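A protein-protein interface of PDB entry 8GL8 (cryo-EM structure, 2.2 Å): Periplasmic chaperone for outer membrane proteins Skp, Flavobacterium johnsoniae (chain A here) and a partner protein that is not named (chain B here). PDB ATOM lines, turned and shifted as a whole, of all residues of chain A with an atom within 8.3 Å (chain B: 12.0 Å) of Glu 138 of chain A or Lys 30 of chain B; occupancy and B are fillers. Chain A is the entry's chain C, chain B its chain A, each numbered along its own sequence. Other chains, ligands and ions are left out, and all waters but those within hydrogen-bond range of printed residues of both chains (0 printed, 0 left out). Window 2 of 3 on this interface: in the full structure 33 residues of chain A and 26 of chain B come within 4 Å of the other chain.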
ATOM      1  N   THR A 131      17.828 -23.990 -22.133  1.00  0.00           N
ATOM      2  CA  THR A 131      19.139 -23.584 -21.641  1.00  0.00           C
ATOM      3  C   THR A 131      19.580 -22.277 -22.283  1.00  0.00           C
ATOM      4  O   THR A 131      20.063 -21.370 -21.595  1.00  0.00           O
ATOM      5  CB  THR A 131      20.164 -24.686 -21.907  1.00  0.00           C
ATOM      6  OG1 THR A 131      19.702 -25.916 -21.337  1.00  0.00           O
ATOM      7  CG2 THR A 131      21.504 -24.324 -21.290  1.00  0.00           C
ATOM      8  N   ALA A 132      19.401 -22.154 -23.602  1.00  0.00           N
ATOM      9  CA  ALA A 132      19.749 -20.901 -24.268  1.00  0.00           C
ATOM     10  C   ALA A 132      18.904 -19.743 -23.749  1.00  0.00           C
ATOM     11  O   ALA A 132      19.426 -18.654 -23.464  1.00  0.00           O
ATOM     12  CB  ALA A 132      19.585 -21.048 -25.779  1.00  0.00           C
ATOM     13  N   VAL A 133      17.595 -19.967 -23.604  1.00  0.00           N
ATOM     14  CA  VAL A 133      16.701 -18.907 -23.145  1.00  0.00           C
ATOM     15  C   VAL A 133      17.048 -18.492 -21.723  1.00  0.00           C
ATOM     16  O   VAL A 133      17.049 -17.302 -21.396  1.00  0.00           O
ATOM     17  CB  VAL A 133      15.232 -19.353 -23.264  1.00  0.00           C
ATOM     18  CG1 VAL A 133      14.320 -18.352 -22.587  1.00  0.00           C
ATOM     19  CG2 VAL A 133      14.847 -19.512 -24.720  1.00  0.00           C
ATOM     20  N   GLN A 134      17.345 -19.461 -20.854  1.00  0.00           N
ATOM     21  CA  GLN A 134      17.713 -19.142 -19.481  1.00  0.00           C
ATOM     22  C   GLN A 134      19.029 -18.381 -19.423  1.00  0.00           C
ATOM     23  O   GLN A 134      19.169 -17.439 -18.636  1.00  0.00           O
ATOM     24  CB  GLN A 134      17.795 -20.421 -18.651  1.00  0.00           C
ATOM     25  CG  GLN A 134      18.072 -20.185 -17.181  1.00  0.00           C
ATOM     26  CD  GLN A 134      17.401 -21.212 -16.295  1.00  0.00           C
ATOM     27  OE1 GLN A 134      16.815 -22.179 -16.780  1.00  0.00           O
ATOM     28  NE2 GLN A 134      17.483 -21.007 -14.985  1.00  0.00           N
ATOM     29  N   ASP A 135      20.005 -18.772 -20.245  1.00  0.00           N
ATOM     30  CA  ASP A 135      21.267 -18.042 -20.281  1.00  0.00           C
ATOM     31  C   ASP A 135      21.043 -16.590 -20.677  1.00  0.00           C
ATOM     32  O   ASP A 135      21.556 -15.669 -20.028  1.00  0.00           O
ATOM     33  CB  ASP A 135      22.237 -18.720 -21.250  1.00  0.00           C
ATOM     34  CG  ASP A 135      22.863 -19.970 -20.669  1.00  0.00           C
ATOM     35  OD1 ASP A 135      22.563 -20.300 -19.501  1.00  0.00           O
ATOM     36  OD2 ASP A 135      23.656 -20.623 -21.378  1.00  0.00           O
ATOM     37  N   ILE A 136      20.252 -16.363 -21.728  1.00  0.00           N
ATOM     38  CA  ILE A 136      20.018 -14.997 -22.184  1.00  0.00           C
ATOM     39  C   ILE A 136      19.212 -14.209 -21.156  1.00  0.00           C
ATOM     40  O   ILE A 136      19.479 -13.027 -20.913  1.00  0.00           O
ATOM     41  CB  ILE A 136      19.340 -15.007 -23.565  1.00  0.00           C
ATOM     42  CG1 ILE A 136      20.372 -15.343 -24.635  1.00  0.00           C
ATOM     43  CG2 ILE A 136      18.699 -13.666 -23.863  1.00  0.00           C
ATOM     44  CD1 ILE A 136      19.775 -15.833 -25.910  1.00  0.00           C
ATOM     45  N   ALA A 137      18.220 -14.848 -20.530  1.00  0.00           N
ATOM     46  CA  ALA A 137      17.405 -14.161 -19.535  1.00  0.00           C
ATOM     47  C   ALA A 137      18.234 -13.756 -18.324  1.00  0.00           C
ATOM     48  O   ALA A 137      18.063 -12.657 -17.787  1.00  0.00           O
ATOM     49  CB  ALA A 137      16.235 -15.048 -19.112  1.00  0.00           C
ATOM     50  N   GLU A 138      19.129 -14.635 -17.870  1.00  0.00           N
ATOM     51  CA  GLU A 138      20.008 -14.281 -16.763  1.00  0.00           C
ATOM     52  C   GLU A 138      20.987 -13.185 -17.164  1.00  0.00           C
ATOM     53  O   GLU A 138      21.286 -12.291 -16.364  1.00  0.00           O
ATOM     54  CB  GLU A 138      20.755 -15.517 -16.265  1.00  0.00           C
ATOM     55  CG  GLU A 138      19.853 -16.586 -15.677  1.00  0.00           C
ATOM     56  CD  GLU A 138      20.280 -17.011 -14.288  1.00  0.00           C
ATOM     57  OE1 GLU A 138      20.967 -16.220 -13.609  1.00  0.00           O
ATOM     58  OE2 GLU A 138      19.929 -18.137 -13.876  1.00  0.00           O
ATOM     59  N   ALA A 139      21.499 -13.237 -18.396  1.00  0.00           N
ATOM     60  CA  ALA A 139      22.437 -12.215 -18.848  1.00  0.00           C
ATOM     61  C   ALA A 139      21.779 -10.842 -18.920  1.00  0.00           C
ATOM     62  O   ALA A 139      22.373  -9.840 -18.509  1.00  0.00           O
ATOM     63  CB  ALA A 139      23.019 -12.600 -20.207  1.00  0.00           C
ATOM     64  N   LYS A 140      20.553 -10.776 -19.437  1.00  0.00           N
ATOM     65  CA  LYS A 140      19.866  -9.510 -19.655  1.00  0.00           C
ATOM     66  C   LYS A 140      18.914  -9.135 -18.527  1.00  0.00           C
ATOM     67  O   LYS A 140      18.206  -8.131 -18.646  1.00  0.00           O
ATOM     68  CB  LYS A 140      19.105  -9.550 -20.981  1.00  0.00           C
ATOM     69  CG  LYS A 140      20.006  -9.548 -22.201  1.00  0.00           C
ATOM     70  CD  LYS A 140      19.202  -9.610 -23.485  1.00  0.00           C
ATOM     71  CE  LYS A 140      19.786  -8.685 -24.537  1.00  0.00           C
ATOM     72  NZ  LYS A 140      21.275  -8.717 -24.524  1.00  0.00           N
ATOM     73  N   ASN A 141      18.875  -9.918 -17.449  1.00  0.00           N
ATOM     74  CA  ASN A 141      18.074  -9.606 -16.264  1.00  0.00           C
ATOM     75  C   ASN A 141      16.586  -9.503 -16.597  1.00  0.00           C
ATOM     76  O   ASN A 141      15.911  -8.537 -16.239  1.00  0.00           O
ATOM     77  CB  ASN A 141      18.572  -8.327 -15.586  1.00  0.00           C
ATOM     78  CG  ASN A 141      19.611  -8.602 -14.519  1.00  0.00           C
ATOM     79  OD1 ASN A 141      19.286  -9.061 -13.425  1.00  0.00           O
ATOM     80  ND2 ASN A 141      20.869  -8.321 -14.833  1.00  0.00           N
ATOM     81  N   TYR A 142      16.075 -10.515 -17.289  1.00  0.00           N
ATOM     82  CA  TYR A 142      14.647 -10.618 -17.556  1.00  0.00           C
ATOM     83  C   TYR A 142      13.967 -11.381 -16.431  1.00  0.00           C
ATOM     84  O   TYR A 142      14.471 -12.407 -15.966  1.00  0.00           O
ATOM     85  CB  TYR A 142      14.388 -11.318 -18.889  1.00  0.00           C
ATOM     86  CG  TYR A 142      14.656 -10.462 -20.103  1.00  0.00           C
ATOM     87  CD1 TYR A 142      14.009  -9.251 -20.276  1.00  0.00           C
ATOM     88  CD2 TYR A 142      15.548 -10.871 -21.079  1.00  0.00           C
ATOM     89  CE1 TYR A 142      14.249  -8.468 -21.384  1.00  0.00           C
ATOM     90  CE2 TYR A 142      15.793 -10.097 -22.190  1.00  0.00           C
ATOM     91  CZ  TYR A 142      15.141  -8.896 -22.338  1.00  0.00           C
ATOM     92  OH  TYR A 142      15.385  -8.122 -23.447  1.00  0.00           O
ATOM     93  N   ASP A 143      12.819 -10.873 -15.990  1.00  0.00           N
ATOM     94  CA  ASP A 143      12.043 -11.529 -14.949  1.00  0.00           C
ATOM     95  C   ASP A 143      10.995 -12.481 -15.499  1.00  0.00           C
ATOM     96  O   ASP A 143      10.712 -13.504 -14.870  1.00  0.00           O
ATOM     97  CB  ASP A 143      11.361 -10.485 -14.060  1.00  0.00           C
ATOM     98  CG  ASP A 143      12.353  -9.566 -13.380  1.00  0.00           C
ATOM     99  OD1 ASP A 143      12.843  -9.919 -12.289  1.00  0.00           O
ATOM    100  OD2 ASP A 143      12.648  -8.489 -13.938  1.00  0.00           O
ATOM    101  N   ILE A 145       9.621 -14.316 -19.372  1.00  0.00           N
ATOM    102  CA  ILE A 145       9.871 -14.559 -20.789  1.00  0.00           C
ATOM    103  C   ILE A 145       8.604 -15.189 -21.351  1.00  0.00           C
ATOM    104  O   ILE A 145       8.374 -16.391 -21.186  1.00  0.00           O
ATOM    105  CB  ILE A 145      11.090 -15.453 -21.032  1.00  0.00           C
ATOM    106  CG1 ILE A 145      12.354 -14.792 -20.478  1.00  0.00           C
ATOM    107  CG2 ILE A 145      11.246 -15.751 -22.514  1.00  0.00           C
ATOM    108  CD1 ILE A 145      13.024 -13.839 -21.437  1.00  0.00           C
ATOM    109  N   ILE A 163      14.109 -11.770 -27.883  1.00  0.00           N
ATOM    110  CA  ILE A 163      15.378 -12.468 -27.763  1.00  0.00           C
ATOM    111  C   ILE A 163      15.394 -13.736 -28.615  1.00  0.00           C
ATOM    112  O   ILE A 163      16.190 -14.635 -28.366  1.00  0.00           O
ATOM    113  CB  ILE A 163      15.706 -12.769 -26.294  1.00  0.00           C
ATOM    114  CG1 ILE A 163      14.623 -13.648 -25.674  1.00  0.00           C
ATOM    115  CG2 ILE A 163      15.828 -11.481 -25.510  1.00  0.00           C
ATOM    116  CD1 ILE A 163      15.080 -14.399 -24.453  1.00  0.00           C
ATOM    117  N   LYS B  30      22.092 -16.088 -10.020  1.00  0.00           N
ATOM    118  CA  LYS B  30      20.966 -17.001 -10.195  1.00  0.00           C
ATOM    119  C   LYS B  30      19.661 -16.372  -9.707  1.00  0.00           C
ATOM    120  O   LYS B  30      19.648 -15.617  -8.734  1.00  0.00           O
ATOM    121  CB  LYS B  30      21.228 -18.338  -9.482  1.00  0.00           C
ATOM    122  CG  LYS B  30      21.041 -18.375  -7.954  1.00  0.00           C
ATOM    123  CD  LYS B  30      21.780 -17.277  -7.198  1.00  0.00           C
ATOM    124  CE  LYS B  30      21.948 -17.639  -5.732  1.00  0.00           C
ATOM    125  NZ  LYS B  30      22.807 -16.662  -5.008  1.00  0.00           N
ATOM    126  N   THR B  31      18.563 -16.668 -10.407  1.00  0.00           N
ATOM    127  CA  THR B  31      17.266 -16.094 -10.075  1.00  0.00           C
ATOM    128  C   THR B  31      16.172 -17.129  -9.848  1.00  0.00           C
ATOM    129  O   THR B  31      15.050 -16.742  -9.502  1.00  0.00           O
ATOM    130  CB  THR B  31      16.804 -15.121 -11.173  1.00  0.00           C
ATOM    131  OG1 THR B  31      16.170 -15.853 -12.226  1.00  0.00           O
ATOM    132  CG2 THR B  31      17.978 -14.339 -11.741  1.00  0.00           C
ATOM    133  N   GLN B  32      16.458 -18.421 -10.030  1.00  0.00           N
ATOM    134  CA  GLN B  32      15.503 -19.502  -9.776  1.00  0.00           C
ATOM    135  C   GLN B  32      14.235 -19.334 -10.617  1.00  0.00           C
ATOM    136  O   GLN B  32      13.140 -19.104 -10.110  1.00  0.00           O
ATOM    137  CB  GLN B  32      15.158 -19.591  -8.282  1.00  0.00           C
ATOM    138  CG  GLN B  32      16.006 -20.573  -7.496  1.00  0.00           C
ATOM    139  CD  GLN B  32      17.441 -20.608  -7.968  1.00  0.00           C
ATOM    140  OE1 GLN B  32      18.168 -19.624  -7.844  1.00  0.00           O
ATOM    141  NE2 GLN B  32      17.859 -21.744  -8.513  1.00  0.00           N
ATOM    142  N   PHE B  33      14.416 -19.448 -11.929  1.00  0.00           N
ATOM    143  CA  PHE B  33      13.287 -19.344 -12.842  1.00  0.00           C
ATOM    144  C   PHE B  33      12.333 -20.523 -12.677  1.00  0.00           C
ATOM    145  O   PHE B  33      12.739 -21.645 -12.365  1.00  0.00           O
ATOM    146  CB  PHE B  33      13.770 -19.276 -14.289  1.00  0.00           C
ATOM    147  CG  PHE B  33      14.352 -17.949 -14.672  1.00  0.00           C
ATOM    148  CD1 PHE B  33      13.531 -16.859 -14.889  1.00  0.00           C
ATOM    149  CD2 PHE B  33      15.717 -17.796 -14.826  1.00  0.00           C
ATOM    150  CE1 PHE B  33      14.059 -15.638 -15.246  1.00  0.00           C
ATOM    151  CE2 PHE B  33      16.252 -16.578 -15.186  1.00  0.00           C
ATOM    152  CZ  PHE B  33      15.422 -15.498 -15.394  1.00  0.00           C
ATOM    153  N   SER B  34      11.044 -20.252 -12.887  1.00  0.00           N
ATOM    154  CA  SER B  34      10.009 -21.283 -12.919  1.00  0.00           C
ATOM    155  C   SER B  34       9.773 -21.643 -14.381  1.00  0.00           C
ATOM    156  O   SER B  34       9.053 -20.945 -15.098  1.00  0.00           O
ATOM    157  CB  SER B  34       8.729 -20.803 -12.246  1.00  0.00           C
ATOM    158  OG  SER B  34       8.972 -20.410 -10.909  1.00  0.00           O
ATOM    159  N   VAL B  35      10.378 -22.739 -14.813  1.00  0.00           N
ATOM    160  CA  VAL B  35      10.398 -23.114 -16.221  1.00  0.00           C
ATOM    161  C   VAL B  35       9.034 -23.649 -16.636  1.00  0.00           C
ATOM    162  O   VAL B  35       8.401 -24.420 -15.907  1.00  0.00           O
ATOM    163  CB  VAL B  35      11.514 -24.142 -16.473  1.00  0.00           C
ATOM    164  CG1 VAL B  35      11.181 -25.033 -17.651  1.00  0.00           C
ATOM    165  CG2 VAL B  35      12.838 -23.436 -16.694  1.00  0.00           C
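Printed residues of chain B that touch a printed residue of chain A: Lys 30, Thr 31 and Phe 33.
Hydrophobic or aromatic side chains of chain B within 4 Å of the printed part of chain A: Phe 33.
Along chain B the printed residues that touch a printed residue of chain A span positions 30 to 33.
Printed residues of chain A that touch a printed residue of chain B: Gln 134, Ala 137, Glu 138, Tyr 142 and Asp 143.
Among the printed residues, no Asp or Glu carboxylate lies within 4 Å of a Lys or Arg side-chain nitrogen of the other chain.
Printed residues of chain B within 4 Å of Gln 134 of chain A: Phe 33.
Ala 137 of chain A touches one residue of chain B.
Of the printed residues of chain B, Glu 138 of chain A touches Lys 30, Thr 31 and Phe 33.
No residue of chain B comes within 4 Å of Ala 139 of chain A.
No residue of chain B comes within 4 Å of Asn 141 of chain A.
Printed residues of chain B within 4 Å of Asp 143 of chain A: Phe 33 (3.99 Å).
Of chain A, only Glu 138 (3.5 Å) comes within 4 Å of Lys 30 of chain B.
Printed residues of chain A within 4 Å of Phe 33 of chain B: Gln 134 (3.7 Å), Ala 137 (3.8 Å), Glu 138 (3.6 Å), Tyr 142 (3.3 Å) and Asp 143 (3.99 Å).
The nearest residue of chain A that does not touch Lys 30 of chain B is Gln 134 of chain A (7.2 Å).
The nearest printed residue of chain A that does not touch Phe 33 of chain B is Ile 145 of chain A (5.6 Å).
O of Ala 137 of chain A lies within hydrogen-bond range of N of Tyr 142 of chain A (3.0 Å).
Among the printed residues, merely in contact across the chains: Gln 134 of chain A with Phe 33 of chain B (3.7 Å), Ala 137 of chain A with Phe 33 of chain B (3.8 Å), Glu 138 of chain A with Lys 30 of chain B (3.5 Å), Glu 138 of chain A with Thr 31 of chain B (3.995 Å), Glu 138 of chain A with Phe 33 of chain B (3.6 Å), Tyr 142 of chain A with Phe 33 of chain B (3.3 Å) and Asp 143 of chain A with Phe 33 of chain B (3.99 Å).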
